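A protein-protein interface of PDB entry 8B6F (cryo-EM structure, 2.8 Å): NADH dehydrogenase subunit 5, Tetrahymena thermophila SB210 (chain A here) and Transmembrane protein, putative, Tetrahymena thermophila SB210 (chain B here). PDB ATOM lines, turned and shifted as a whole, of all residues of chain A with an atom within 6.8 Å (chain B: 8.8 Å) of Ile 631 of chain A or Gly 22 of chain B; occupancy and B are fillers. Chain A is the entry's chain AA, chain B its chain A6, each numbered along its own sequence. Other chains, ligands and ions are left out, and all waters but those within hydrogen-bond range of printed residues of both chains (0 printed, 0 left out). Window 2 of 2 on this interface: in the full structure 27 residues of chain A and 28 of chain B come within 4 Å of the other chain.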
ATOM      1  N   ALA A 628      -7.681 -17.252  -7.653  1.00  0.00           N
ATOM      2  CA  ALA A 628      -7.655 -18.469  -8.453  1.00  0.00           C
ATOM      3  C   ALA A 628      -6.731 -18.385  -9.661  1.00  0.00           C
ATOM      4  O   ALA A 628      -6.446 -19.421 -10.269  1.00  0.00           O
ATOM      5  CB  ALA A 628      -9.071 -18.812  -8.930  1.00  0.00           C
ATOM      6  N   SER A 629      -6.270 -17.192 -10.031  1.00  0.00           N
ATOM      7  CA  SER A 629      -5.392 -17.024 -11.182  1.00  0.00           C
ATOM      8  C   SER A 629      -3.911 -17.151 -10.844  1.00  0.00           C
ATOM      9  O   SER A 629      -3.076 -16.971 -11.736  1.00  0.00           O
ATOM     10  CB  SER A 629      -5.647 -15.665 -11.840  1.00  0.00           C
ATOM     11  OG  SER A 629      -5.333 -14.602 -10.959  1.00  0.00           O
ATOM     12  N   ARG A 630      -3.559 -17.455  -9.599  1.00  0.00           N
ATOM     13  CA  ARG A 630      -2.154 -17.536  -9.220  1.00  0.00           C
ATOM     14  C   ARG A 630      -1.476 -18.708  -9.920  1.00  0.00           C
ATOM     15  O   ARG A 630      -2.024 -19.809  -9.997  1.00  0.00           O
ATOM     16  CB  ARG A 630      -2.018 -17.678  -7.705  1.00  0.00           C
ATOM     17  CG  ARG A 630      -2.723 -16.590  -6.900  1.00  0.00           C
ATOM     18  CD  ARG A 630      -2.205 -15.200  -7.238  1.00  0.00           C
ATOM     19  NE  ARG A 630      -2.762 -14.688  -8.485  1.00  0.00           N
ATOM     20  CZ  ARG A 630      -2.424 -13.533  -9.039  1.00  0.00           C
ATOM     21  NH1 ARG A 630      -1.527 -12.736  -8.484  1.00  0.00           N
ATOM     22  NH2 ARG A 630      -2.999 -13.168 -10.181  1.00  0.00           N
ATOM     23  N   ILE A 631      -0.260 -18.466 -10.419  1.00  0.00           N
ATOM     24  CA  ILE A 631       0.442 -19.482 -11.200  1.00  0.00           C
ATOM     25  C   ILE A 631       0.773 -20.699 -10.351  1.00  0.00           C
ATOM     26  O   ILE A 631       0.872 -21.816 -10.870  1.00  0.00           O
ATOM     27  CB  ILE A 631       1.713 -18.890 -11.843  1.00  0.00           C
ATOM     28  CG1 ILE A 631       2.655 -18.338 -10.768  1.00  0.00           C
ATOM     29  CG2 ILE A 631       1.337 -17.813 -12.850  1.00  0.00           C
ATOM     30  CD1 ILE A 631       3.974 -17.822 -11.308  1.00  0.00           C
ATOM     31  N   ILE A 632       0.961 -20.511  -9.044  1.00  0.00           N
ATOM     32  CA  ILE A 632       1.308 -21.635  -8.178  1.00  0.00           C
ATOM     33  C   ILE A 632       0.234 -22.712  -8.240  1.00  0.00           C
ATOM     34  O   ILE A 632       0.525 -23.900  -8.062  1.00  0.00           O
ATOM     35  CB  ILE A 632       1.530 -21.142  -6.734  1.00  0.00           C
ATOM     36  CG1 ILE A 632       1.996 -22.284  -5.827  1.00  0.00           C
ATOM     37  CG2 ILE A 632       0.256 -20.521  -6.174  1.00  0.00           C
ATOM     38  CD1 ILE A 632       3.371 -22.811  -6.157  1.00  0.00           C
ATOM     39  N   LEU A 633      -1.015 -22.323  -8.493  1.00  0.00           N
ATOM     40  CA  LEU A 633      -2.116 -23.274  -8.528  1.00  0.00           C
ATOM     41  C   LEU A 633      -2.130 -24.121  -9.792  1.00  0.00           C
ATOM     42  O   LEU A 633      -2.822 -25.143  -9.824  1.00  0.00           O
ATOM     43  CB  LEU A 633      -3.447 -22.531  -8.399  1.00  0.00           C
ATOM     44  CG  LEU A 633      -3.616 -21.703  -7.126  1.00  0.00           C
ATOM     45  CD1 LEU A 633      -4.904 -20.902  -7.178  1.00  0.00           C
ATOM     46  CD2 LEU A 633      -3.591 -22.591  -5.895  1.00  0.00           C
ATOM     47  N   ASN A 634      -1.390 -23.728 -10.828  1.00  0.00           N
ATOM     48  CA  ASN A 634      -1.381 -24.480 -12.076  1.00  0.00           C
ATOM     49  C   ASN A 634      -0.919 -25.906 -11.821  1.00  0.00           C
ATOM     50  O   ASN A 634       0.244 -26.137 -11.478  1.00  0.00           O
ATOM     51  CB  ASN A 634      -0.475 -23.803 -13.107  1.00  0.00           C
ATOM     52  CG  ASN A 634      -0.626 -24.397 -14.492  1.00  0.00           C
ATOM     53  OD1 ASN A 634      -0.987 -25.563 -14.645  1.00  0.00           O
ATOM     54  ND2 ASN A 634      -0.352 -23.594 -15.513  1.00  0.00           N
ATOM     55  N   SER A 635      -1.818 -26.871 -11.992  1.00  0.00           N
ATOM     56  CA  SER A 635      -1.497 -28.259 -11.702  1.00  0.00           C
ATOM     57  C   SER A 635      -2.498 -29.157 -12.409  1.00  0.00           C
ATOM     58  O   SER A 635      -3.558 -28.708 -12.853  1.00  0.00           O
ATOM     59  CB  SER A 635      -1.510 -28.527 -10.193  1.00  0.00           C
ATOM     60  OG  SER A 635      -1.208 -29.881  -9.914  1.00  0.00           O
ATOM     61  N   GLY B  22       7.560 -19.346  -9.302  1.00  0.00           N
ATOM     62  CA  GLY B  22       6.237 -19.570  -8.657  1.00  0.00           C
ATOM     63  C   GLY B  22       5.599 -20.884  -9.061  1.00  0.00           C
ATOM     64  O   GLY B  22       4.815 -21.456  -8.308  1.00  0.00           O
ATOM     65  N   ASP B  23       5.936 -21.364 -10.255  1.00  0.00           N
ATOM     66  CA  ASP B  23       5.395 -22.613 -10.769  1.00  0.00           C
ATOM     67  C   ASP B  23       6.257 -23.776 -10.295  1.00  0.00           C
ATOM     68  O   ASP B  23       7.488 -23.714 -10.371  1.00  0.00           O
ATOM     69  CB  ASP B  23       5.338 -22.579 -12.297  1.00  0.00           C
ATOM     70  CG  ASP B  23       4.507 -23.705 -12.874  1.00  0.00           C
ATOM     71  OD1 ASP B  23       3.911 -24.468 -12.087  1.00  0.00           O
ATOM     72  OD2 ASP B  23       4.451 -23.826 -14.115  1.00  0.00           O
ATOM     73  N   ILE B  24       5.609 -24.833  -9.811  1.00  0.00           N
ATOM     74  CA  ILE B  24       6.299 -25.986  -9.248  1.00  0.00           C
ATOM     75  C   ILE B  24       5.922 -27.276  -9.975  1.00  0.00           C
ATOM     76  O   ILE B  24       6.113 -28.363  -9.446  1.00  0.00           O
ATOM     77  CB  ILE B  24       6.031 -26.105  -7.736  1.00  0.00           C
ATOM     78  CG1 ILE B  24       4.535 -26.301  -7.475  1.00  0.00           C
ATOM     79  CG2 ILE B  24       6.546 -24.863  -7.018  1.00  0.00           C
ATOM     80  CD1 ILE B  24       4.174 -26.477  -6.015  1.00  0.00           C
ATOM     81  N   ARG B  25       5.383 -27.166 -11.191  1.00  0.00           N
ATOM     82  CA  ARG B  25       5.010 -28.359 -11.941  1.00  0.00           C
ATOM     83  C   ARG B  25       6.225 -29.204 -12.301  1.00  0.00           C
ATOM     84  O   ARG B  25       6.107 -30.425 -12.450  1.00  0.00           O
ATOM     85  CB  ARG B  25       4.251 -27.965 -13.207  1.00  0.00           C
ATOM     86  CG  ARG B  25       2.838 -27.475 -12.948  1.00  0.00           C
ATOM     87  CD  ARG B  25       2.381 -26.519 -14.035  1.00  0.00           C
ATOM     88  NE  ARG B  25       2.556 -27.077 -15.369  1.00  0.00           N
ATOM     89  CZ  ARG B  25       2.432 -26.385 -16.493  1.00  0.00           C
ATOM     90  NH1 ARG B  25       2.141 -25.095 -16.481  1.00  0.00           N
ATOM     91  NH2 ARG B  25       2.610 -27.001 -17.657  1.00  0.00           N
ATOM     92  N   HIS B  26       7.394 -28.581 -12.440  1.00  0.00           N
ATOM     93  CA  HIS B  26       8.589 -29.318 -12.834  1.00  0.00           C
ATOM     94  C   HIS B  26       9.095 -30.242 -11.733  1.00  0.00           C
ATOM     95  O   HIS B  26       9.867 -31.160 -12.023  1.00  0.00           O
ATOM     96  CB  HIS B  26       9.697 -28.343 -13.234  1.00  0.00           C
ATOM     97  CG  HIS B  26      10.092 -27.401 -12.142  1.00  0.00           C
ATOM     98  ND1 HIS B  26       9.479 -26.180 -11.954  1.00  0.00           N
ATOM     99  CD2 HIS B  26      11.035 -27.499 -11.177  1.00  0.00           C
ATOM    100  CE1 HIS B  26      10.029 -25.568 -10.922  1.00  0.00           C
ATOM    101  NE2 HIS B  26      10.976 -26.346 -10.432  1.00  0.00           N
ATOM    102  N   LYS B  27       8.684 -30.022 -10.484  1.00  0.00           N
ATOM    103  CA  LYS B  27       9.163 -30.842  -9.378  1.00  0.00           C
ATOM    104  C   LYS B  27       8.574 -32.246  -9.376  1.00  0.00           C
ATOM    105  O   LYS B  27       9.047 -33.091  -8.610  1.00  0.00           O
ATOM    106  CB  LYS B  27       8.850 -30.161  -8.046  1.00  0.00           C
ATOM    107  CG  LYS B  27       9.620 -28.872  -7.818  1.00  0.00           C
ATOM    108  CD  LYS B  27       9.265 -28.247  -6.480  1.00  0.00           C
ATOM    109  CE  LYS B  27      10.134 -27.033  -6.193  1.00  0.00           C
ATOM    110  NZ  LYS B  27      10.069 -26.022  -7.283  1.00  0.00           N
ATOM    111  N   TYR B  37      -1.544 -29.384 -22.329  1.00  0.00           N
ATOM    112  CA  TYR B  37      -2.452 -28.250 -22.457  1.00  0.00           C
ATOM    113  C   TYR B  37      -2.631 -27.784 -23.896  1.00  0.00           C
ATOM    114  O   TYR B  37      -3.499 -26.943 -24.148  1.00  0.00           O
ATOM    115  CB  TYR B  37      -1.946 -27.073 -21.616  1.00  0.00           C
ATOM    116  CG  TYR B  37      -2.314 -27.125 -20.148  1.00  0.00           C
ATOM    117  CD1 TYR B  37      -3.606 -27.425 -19.741  1.00  0.00           C
ATOM    118  CD2 TYR B  37      -1.365 -26.860 -19.171  1.00  0.00           C
ATOM    119  CE1 TYR B  37      -3.940 -27.466 -18.403  1.00  0.00           C
ATOM    120  CE2 TYR B  37      -1.690 -26.898 -17.830  1.00  0.00           C
ATOM    121  CZ  TYR B  37      -2.979 -27.200 -17.454  1.00  0.00           C
ATOM    122  OH  TYR B  37      -3.306 -27.241 -16.119  1.00  0.00           O
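The side-chain amide oxygen of Asn 634 of chain A lies within hydrogen-bond range of the side-chain hydroxyl of Tyr 37 of chain B (3.2 Å). NH1 of Arg 25 of chain B lies close to ND2 of Asn 634 of chain A.
NH1 of Arg 25 of chain B lies within salt-bridge range of OD2 of Asp 23 of chain B, 3.5 Å away.
CD1 of Ile 631 of chain A touches CA of Gly 22 of chain B, at 3.9 Å. Gly 22 of chain B touches Ile 632 of chain A. Ile 24 of chain B touches Ile 632 of chain A (CD1 to CD1, 3.8 Å). Ser 635 of chain A touches Tyr 37 of chain B (O to OH, 3.6 Å).
Of chain B, only Gly 22 comes within 4 Å of Ile 631 of chain A. Of chain A, only Ile 631 and Ile 632 come within 4 Å of Gly 22 of chain B. Of the printed residues of chain A, Tyr 37 of chain B touches Asn 634 and Ser 635. Printed residues of chain A within 4 Å of Ile 24 of chain B: Ile 632. Printed residues of chain B within 4 Å of Asn 634 of chain A: Arg 25 (3.1 Å) and Tyr 37 (3.2 Å).
Printed residues of chain A that touch a printed residue of chain B: Ile 631, Ile 632, Asn 634 and Ser 635. Hydrophobic or aromatic side chains of chain A that line the printed part of chain B: Ile 631 and Ile 632. Of the 7 printed residues of chain B, 4 touch a printed residue of chain A. Printed residues of chain B that touch a printed residue of chain A: Gly 22, Ile 24, Arg 25 and Tyr 37. Hydrophobic or aromatic side chains of chain B that line the printed part of chain A: Ile 24 and Tyr 37. Among the printed residues, no Asp or Glu carboxylate lies within 4 Å of a Lys or Arg side-chain nitrogen of the other chain.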
